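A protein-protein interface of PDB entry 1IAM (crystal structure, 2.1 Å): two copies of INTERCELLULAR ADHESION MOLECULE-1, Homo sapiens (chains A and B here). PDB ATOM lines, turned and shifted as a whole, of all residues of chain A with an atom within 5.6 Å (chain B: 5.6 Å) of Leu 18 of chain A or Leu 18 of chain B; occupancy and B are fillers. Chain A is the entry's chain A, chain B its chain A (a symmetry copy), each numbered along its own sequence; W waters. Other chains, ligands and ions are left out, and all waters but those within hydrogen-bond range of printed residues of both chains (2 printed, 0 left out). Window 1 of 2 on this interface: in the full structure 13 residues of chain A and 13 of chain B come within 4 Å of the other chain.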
ATOM      1  N   SER A   5     -17.292   4.431  12.581  1.00  0.00           N
ATOM      2  CA  SER A   5     -17.233   3.434  11.534  1.00  0.00           C
ATOM      3  C   SER A   5     -18.646   2.849  11.424  1.00  0.00           C
ATOM      4  O   SER A   5     -19.233   2.466  12.440  1.00  0.00           O
ATOM      5  CB  SER A   5     -16.192   2.375  11.908  1.00  0.00           C
ATOM      6  OG  SER A   5     -16.213   1.256  11.032  1.00  0.00           O
ATOM      7  N   PRO A   6     -19.249   2.862  10.208  1.00  0.00           N
ATOM      8  CA  PRO A   6     -18.722   3.378   8.935  1.00  0.00           C
ATOM      9  C   PRO A   6     -18.789   4.903   8.891  1.00  0.00           C
ATOM     10  O   PRO A   6     -19.668   5.492   9.516  1.00  0.00           O
ATOM     11  CB  PRO A   6     -19.702   2.812   7.898  1.00  0.00           C
ATOM     12  CG  PRO A   6     -20.546   1.818   8.626  1.00  0.00           C
ATOM     13  CD  PRO A   6     -20.620   2.357  10.016  1.00  0.00           C
ATOM     14  N   SER A  16     -32.196   0.616   8.765  1.00  0.00           N
ATOM     15  CA  SER A  16     -31.404   0.725   9.994  1.00  0.00           C
ATOM     16  C   SER A  16     -29.926   0.458   9.709  1.00  0.00           C
ATOM     17  O   SER A  16     -29.591  -0.249   8.756  1.00  0.00           O
ATOM     18  CB  SER A  16     -31.908  -0.294  11.026  1.00  0.00           C
ATOM     19  OG  SER A  16     -33.298  -0.123  11.238  1.00  0.00           O
ATOM     20  N   VAL A  17     -29.057   1.005  10.556  1.00  0.00           N
ATOM     21  CA  VAL A  17     -27.620   0.842  10.411  1.00  0.00           C
ATOM     22  C   VAL A  17     -26.923   0.819  11.778  1.00  0.00           C
ATOM     23  O   VAL A  17     -27.374   1.468  12.729  1.00  0.00           O
ATOM     24  CB  VAL A  17     -27.023   2.002   9.550  1.00  0.00           C
ATOM     25  CG1 VAL A  17     -27.262   3.357  10.227  1.00  0.00           C
ATOM     26  CG2 VAL A  17     -25.527   1.778   9.279  1.00  0.00           C
ATOM     27  N   LEU A  18     -25.840   0.054  11.870  1.00  0.00           N
ATOM     28  CA  LEU A  18     -25.036  -0.039  13.089  1.00  0.00           C
ATOM     29  C   LEU A  18     -23.886   0.943  12.986  1.00  0.00           C
ATOM     30  O   LEU A  18     -23.164   0.931  12.001  1.00  0.00           O
ATOM     31  CB  LEU A  18     -24.464  -1.436  13.261  1.00  0.00           C
ATOM     32  CG  LEU A  18     -25.419  -2.540  13.729  1.00  0.00           C
ATOM     33  CD1 LEU A  18     -24.678  -3.880  13.789  1.00  0.00           C
ATOM     34  CD2 LEU A  18     -25.972  -2.142  15.081  1.00  0.00           C
ATOM     35  N   VAL A  19     -23.708   1.767  14.014  1.00  0.00           N
ATOM     36  CA  VAL A  19     -22.661   2.774  14.060  1.00  0.00           C
ATOM     37  C   VAL A  19     -21.812   2.560  15.321  1.00  0.00           C
ATOM     38  O   VAL A  19     -22.355   2.357  16.413  1.00  0.00           O
ATOM     39  CB  VAL A  19     -23.274   4.191  14.140  1.00  0.00           C
ATOM     40  CG1 VAL A  19     -22.183   5.238  14.088  1.00  0.00           C
ATOM     41  CG2 VAL A  19     -24.288   4.417  13.003  1.00  0.00           C
ATOM     42  N   THR A  20     -20.488   2.574  15.171  1.00  0.00           N
ATOM     43  CA  THR A  20     -19.609   2.407  16.313  1.00  0.00           C
ATOM     44  C   THR A  20     -18.791   3.686  16.520  1.00  0.00           C
ATOM     45  O   THR A  20     -18.142   4.188  15.589  1.00  0.00           O
ATOM     46  CB  THR A  20     -18.664   1.199  16.144  1.00  0.00           C
ATOM     47  OG1 THR A  20     -19.438  -0.005  16.038  1.00  0.00           O
ATOM     48  CG2 THR A  20     -17.691   1.079  17.329  1.00  0.00           C
ATOM     49  N   LEU A  42     -26.029  -0.651  22.193  1.00  0.00           N
ATOM     50  CA  LEU A  42     -25.573  -2.033  22.461  1.00  0.00           C
ATOM     51  C   LEU A  42     -24.304  -1.955  23.332  1.00  0.00           C
ATOM     52  O   LEU A  42     -23.883  -0.872  23.720  1.00  0.00           O
ATOM     53  CB  LEU A  42     -25.233  -2.773  21.167  1.00  0.00           C
ATOM     54  CG  LEU A  42     -26.349  -3.234  20.236  1.00  0.00           C
ATOM     55  CD1 LEU A  42     -26.860  -2.053  19.401  1.00  0.00           C
ATOM     56  CD2 LEU A  42     -25.763  -4.291  19.335  1.00  0.00           C
ATOM     57  N   VAL A  51     -21.663   1.060  20.539  1.00  0.00           N
ATOM     58  CA  VAL A  51     -22.365   0.724  19.311  1.00  0.00           C
ATOM     59  C   VAL A  51     -23.832   1.102  19.431  1.00  0.00           C
ATOM     60  O   VAL A  51     -24.480   0.830  20.455  1.00  0.00           O
ATOM     61  CB  VAL A  51     -22.239  -0.769  18.971  1.00  0.00           C
ATOM     62  CG1 VAL A  51     -22.958  -1.084  17.653  1.00  0.00           C
ATOM     63  CG2 VAL A  51     -20.784  -1.156  18.861  1.00  0.00           C
ATOM     64  N   TYR A  52     -24.349   1.726  18.378  1.00  0.00           N
ATOM     65  CA  TYR A  52     -25.734   2.170  18.326  1.00  0.00           C
ATOM     66  C   TYR A  52     -26.425   1.716  17.059  1.00  0.00           C
ATOM     67  O   TYR A  52     -25.839   1.745  15.981  1.00  0.00           O
ATOM     68  CB  TYR A  52     -25.781   3.690  18.306  1.00  0.00           C
ATOM     69  CG  TYR A  52     -25.029   4.341  19.418  1.00  0.00           C
ATOM     70  CD1 TYR A  52     -23.688   4.666  19.258  1.00  0.00           C
ATOM     71  CD2 TYR A  52     -25.663   4.650  20.635  1.00  0.00           C
ATOM     72  CE1 TYR A  52     -22.985   5.287  20.257  1.00  0.00           C
ATOM     73  CE2 TYR A  52     -24.961   5.275  21.661  1.00  0.00           C
ATOM     74  CZ  TYR A  52     -23.624   5.597  21.455  1.00  0.00           C
ATOM     75  OH  TYR A  52     -22.931   6.285  22.404  1.00  0.00           O
ATOM     76  N   GLU A  53     -27.680   1.327  17.172  1.00  0.00           N
ATOM     77  CA  GLU A  53     -28.430   0.962  15.983  1.00  0.00           C
ATOM     78  C   GLU A  53     -29.360   2.148  15.738  1.00  0.00           C
ATOM     79  O   GLU A  53     -30.086   2.563  16.635  1.00  0.00           O
ATOM     80  CB  GLU A  53     -29.239  -0.322  16.187  1.00  0.00           C
ATOM     81  CG  GLU A  53     -30.102  -0.707  14.990  1.00  0.00           C
ATOM     82  CD  GLU A  53     -30.939  -1.959  15.233  1.00  0.00           C
ATOM     83  OE1 GLU A  53     -31.588  -2.073  16.301  1.00  0.00           O
ATOM     84  OE2 GLU A  53     -30.954  -2.840  14.351  1.00  0.00           O
ATOM     85  N   LEU A  54     -29.202   2.787  14.587  1.00  0.00           N
ATOM     86  CA  LEU A  54     -30.018   3.920  14.190  1.00  0.00           C
ATOM     87  C   LEU A  54     -31.106   3.296  13.340  1.00  0.00           C
ATOM     88  O   LEU A  54     -30.813   2.495  12.475  1.00  0.00           O
ATOM     89  CB  LEU A  54     -29.165   4.912  13.391  1.00  0.00           C
ATOM     90  CG  LEU A  54     -28.515   6.046  14.195  1.00  0.00           C
ATOM     91  CD1 LEU A  54     -28.137   5.604  15.597  1.00  0.00           C
ATOM     92  CD2 LEU A  54     -27.306   6.625  13.432  1.00  0.00           C
ATOM     93  N   SER B   5     -27.449 -10.002   8.342  1.00  0.00           N
ATOM     94  CA  SER B   5     -27.240  -8.707   7.732  1.00  0.00           C
ATOM     95  C   SER B   5     -25.896  -8.198   8.264  1.00  0.00           C
ATOM     96  O   SER B   5     -25.670  -8.216   9.478  1.00  0.00           O
ATOM     97  CB  SER B   5     -28.402  -7.782   8.105  1.00  0.00           C
ATOM     98  OG  SER B   5     -28.175  -6.435   7.713  1.00  0.00           O
ATOM     99  N   PRO B   6     -24.950  -7.831   7.363  1.00  0.00           N
ATOM    100  CA  PRO B   6     -25.033  -7.854   5.895  1.00  0.00           C
ATOM    101  C   PRO B   6     -24.872  -9.275   5.358  1.00  0.00           C
ATOM    102  O   PRO B   6     -24.195 -10.088   5.983  1.00  0.00           O
ATOM    103  CB  PRO B   6     -23.816  -7.024   5.464  1.00  0.00           C
ATOM    104  CG  PRO B   6     -23.291  -6.385   6.707  1.00  0.00           C
ATOM    105  CD  PRO B   6     -23.615  -7.367   7.783  1.00  0.00           C
ATOM    106  N   SER B  16     -12.325  -5.944  10.803  1.00  0.00           N
ATOM    107  CA  SER B  16     -13.449  -6.420  11.616  1.00  0.00           C
ATOM    108  C   SER B  16     -14.781  -5.991  11.001  1.00  0.00           C
ATOM    109  O   SER B  16     -14.847  -4.985  10.292  1.00  0.00           O
ATOM    110  CB  SER B  16     -13.342  -5.841  13.034  1.00  0.00           C
ATOM    111  OG  SER B  16     -12.076  -6.150  13.590  1.00  0.00           O
ATOM    112  N   VAL B  17     -15.836  -6.744  11.303  1.00  0.00           N
ATOM    113  CA  VAL B  17     -17.166  -6.463  10.791  1.00  0.00           C
ATOM    114  C   VAL B  17     -18.248  -6.868  11.801  1.00  0.00           C
ATOM    115  O   VAL B  17     -18.075  -7.824  12.564  1.00  0.00           O
ATOM    116  CB  VAL B  17     -17.406  -7.227   9.448  1.00  0.00           C
ATOM    117  CG1 VAL B  17     -17.312  -8.742   9.663  1.00  0.00           C
ATOM    118  CG2 VAL B  17     -18.758  -6.842   8.825  1.00  0.00           C
ATOM    119  N   LEU B  18     -19.348  -6.121  11.811  1.00  0.00           N
ATOM    120  CA  LEU B  18     -20.490  -6.403  12.681  1.00  0.00           C
ATOM    121  C   LEU B  18     -21.498  -7.227  11.904  1.00  0.00           C
ATOM    122  O   LEU B  18     -21.883  -6.842  10.811  1.00  0.00           O
ATOM    123  CB  LEU B  18     -21.163  -5.119  13.133  1.00  0.00           C
ATOM    124  CG  LEU B  18     -20.460  -4.294  14.217  1.00  0.00           C
ATOM    125  CD1 LEU B  18     -21.256  -3.014  14.499  1.00  0.00           C
ATOM    126  CD2 LEU B  18     -20.326  -5.157  15.454  1.00  0.00           C
ATOM    127  N   VAL B  19     -21.936  -8.340  12.484  1.00  0.00           N
ATOM    128  CA  VAL B  19     -22.889  -9.243  11.863  1.00  0.00           C
ATOM    129  C   VAL B  19     -24.094  -9.425  12.797  1.00  0.00           C
ATOM    130  O   VAL B  19     -23.923  -9.635  14.003  1.00  0.00           O
ATOM    131  CB  VAL B  19     -22.254 -10.635  11.640  1.00  0.00           C
ATOM    132  CG1 VAL B  19     -23.217 -11.541  10.905  1.00  0.00           C
ATOM    133  CG2 VAL B  19     -20.930 -10.517  10.862  1.00  0.00           C
ATOM    134  N   THR B  20     -25.306  -9.314  12.254  1.00  0.00           N
ATOM    135  CA  THR B  20     -26.500  -9.496  13.058  1.00  0.00           C
ATOM    136  C   THR B  20     -27.271 -10.722  12.557  1.00  0.00           C
ATOM    137  O   THR B  20     -27.575 -10.842  11.360  1.00  0.00           O
ATOM    138  CB  THR B  20     -27.413  -8.253  13.028  1.00  0.00           C
ATOM    139  OG1 THR B  20     -26.711  -7.129  13.580  1.00  0.00           O
ATOM    140  CG2 THR B  20     -28.706  -8.490  13.826  1.00  0.00           C
ATOM    141  N   LEU B  42     -22.365  -8.975  21.290  1.00  0.00           N
ATOM    142  CA  LEU B  42     -22.956  -7.743  21.858  1.00  0.00           C
ATOM    143  C   LEU B  42     -24.424  -8.043  22.218  1.00  0.00           C
ATOM    144  O   LEU B  42     -24.883  -9.169  22.067  1.00  0.00           O
ATOM    145  CB  LEU B  42     -22.924  -6.591  20.855  1.00  0.00           C
ATOM    146  CG  LEU B  42     -21.604  -5.903  20.524  1.00  0.00           C
ATOM    147  CD1 LEU B  42     -20.798  -6.756  19.537  1.00  0.00           C
ATOM    148  CD2 LEU B  42     -21.943  -4.572  19.903  1.00  0.00           C
ATOM    149  N   VAL B  51     -25.914  -9.780  17.902  1.00  0.00           N
ATOM    150  CA  VAL B  51     -24.890  -9.086  17.139  1.00  0.00           C
ATOM    151  C   VAL B  51     -23.512  -9.562  17.566  1.00  0.00           C
ATOM    152  O   VAL B  51     -23.223  -9.690  18.768  1.00  0.00           O
ATOM    153  CB  VAL B  51     -24.988  -7.562  17.305  1.00  0.00           C
ATOM    154  CG1 VAL B  51     -23.918  -6.858  16.459  1.00  0.00           C
ATOM    155  CG2 VAL B  51     -26.359  -7.081  16.893  1.00  0.00           C
ATOM    156  N   TYR B  52     -22.664  -9.819  16.576  1.00  0.00           N
ATOM    157  CA  TYR B  52     -21.307 -10.294  16.802  1.00  0.00           C
ATOM    158  C   TYR B  52     -20.287  -9.476  16.041  1.00  0.00           C
ATOM    159  O   TYR B  52     -20.513  -9.105  14.893  1.00  0.00           O
ATOM    160  CB  TYR B  52     -21.172 -11.718  16.282  1.00  0.00           C
ATOM    161  CG  TYR B  52     -22.191 -12.665  16.821  1.00  0.00           C
ATOM    162  CD1 TYR B  52     -23.400 -12.842  16.158  1.00  0.00           C
ATOM    163  CD2 TYR B  52     -21.945 -13.403  17.992  1.00  0.00           C
ATOM    164  CE1 TYR B  52     -24.339 -13.726  16.621  1.00  0.00           C
ATOM    165  CE2 TYR B  52     -22.891 -14.300  18.477  1.00  0.00           C
ATOM    166  CZ  TYR B  52     -24.081 -14.458  17.776  1.00  0.00           C
ATOM    167  OH  TYR B  52     -24.992 -15.389  18.174  1.00  0.00           O
ATOM    168  N   GLU B  53     -19.151  -9.218  16.658  1.00  0.00           N
ATOM    169  CA  GLU B  53     -18.094  -8.513  15.953  1.00  0.00           C
ATOM    170  C   GLU B  53     -17.070  -9.594  15.617  1.00  0.00           C
ATOM    171  O   GLU B  53     -16.631 -10.328  16.496  1.00  0.00           O
ATOM    172  CB  GLU B  53     -17.458  -7.421  16.818  1.00  0.00           C
ATOM    173  CG  GLU B  53     -16.293  -6.700  16.148  1.00  0.00           C
ATOM    174  CD  GLU B  53     -15.640  -5.654  17.046  1.00  0.00           C
ATOM    175  OE1 GLU B  53     -15.356  -5.944  18.233  1.00  0.00           O
ATOM    176  OE2 GLU B  53     -15.405  -4.528  16.565  1.00  0.00           O
ATOM    177  N   LEU B  54     -16.833  -9.795  14.328  1.00  0.00           N
ATOM    178  CA  LEU B  54     -15.874 -10.768  13.840  1.00  0.00           C
ATOM    179  C   LEU B  54     -14.614  -9.953  13.628  1.00  0.00           C
ATOM    180  O   LEU B  54     -14.672  -8.891  13.041  1.00  0.00           O
ATOM    181  CB  LEU B  54     -16.386 -11.381  12.531  1.00  0.00           C
ATOM    182  CG  LEU B  54     -17.187 -12.684  12.662  1.00  0.00           C
ATOM    183  CD1 LEU B  54     -17.999 -12.724  13.943  1.00  0.00           C
ATOM    184  CD2 LEU B  54     -18.071 -12.902  11.417  1.00  0.00           C
HETATM  185  O   HOH W   1     -28.694  -4.662  14.437  1.00  0.00           O
HETATM  186  O   HOH W   2     -17.680  -2.722  16.569  1.00  0.00           O
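N of Thr 20 of chain A sits at hydrogen-bond distance from O of Ser 5 of chain A, 3.0 Å away. O of Val 51 of chain A is in hydrogen-bond range of N of Leu 42 of chain A, at 2.8 Å. The backbone NH of Thr 20 of chain B is in hydrogen-bond range of the backbone carbonyl oxygen of Ser 5 of chain B (3.0 Å). The backbone NH of Leu 42 of chain B is in hydrogen-bond range of the backbone carbonyl oxygen of Val 51 of chain B.
Leu 18 of chain A touches its own counterpart, Leu 18 of chain B. Leu 18 of chain A touches Thr 20 of chain B, and with the chains exchanged Thr 20 of chain A touches Leu 18 of chain B. Leu 42 of chain A touches its own counterpart, Leu 42 of chain B. Leu 42 of chain A touches Val 51 of chain B, and with the chains exchanged Val 51 of chain A touches Leu 42 of chain B. Of the 6 pairs that touch across the chains among the printed residues, 6 have their exchanged pair printed and touching as well.
Of chain B, only Leu 18 and Thr 20 come within 4 Å of Leu 18 of chain A. Of the printed residues of chain B, Thr 20 of chain A touches Leu 18 (3.8 Å). Of the printed residues of chain B, Leu 42 of chain A touches Leu 42 and Val 51. Tyr 52 of chain A touches none of the printed residues of chain B. Leu 18 of chain B touches just these residues of chain A: Leu 18 (3.6 Å) and Thr 20 (3.8 Å). Val 19 of chain B touches none of the printed residues of chain A. Of the printed residues of chain A, Val 51 of chain B touches Leu 42 (3.8 Å). The nearest residue of chain A that does not touch Leu 18 of chain B is Val 51 of chain A (4.1 Å). The nearest printed residue of chain A that does not touch Val 51 of chain B is Leu 18 of chain A (4.1 Å).
Among the printed residues, merely in contact across the chains: Leu 18 of chain A with Leu 18 of chain B, Leu 18 of chain A with Thr 20 of chain B, Thr 20 of chain A with Leu 18 of chain B, Leu 42 of chain A with Leu 42 of chain B, Leu 42 of chain A with Val 51 of chain B and Val 51 of chain A with Leu 42 of chain B.
Water W2 lies within hydrogen-bond range of OE2 of Glu 53 of chain B and OG1 of Thr 20 of chain A. Water W1 bridges OE2 of Glu 53 of chain A and OG1 of Thr 20 of chain B.
Hydrophobic or aromatic side chains of chain A within 4 Å of the printed part of chain B: Leu 18, Leu 42 and Val 51. Along chain A the printed residues that touch a printed residue of chain B span positions 18 to 51. Of the 12 printed residues of chain B, 4 touch a printed residue of chain A. Hydrophobic or aromatic side chains of chain B within 4 Å of the printed part of chain A: Leu 18, Leu 42 and Val 51. Among the printed residues, no Asp or Glu carboxylate lies within 4 Å of a Lys or Arg side-chain nitrogen of the other chain.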
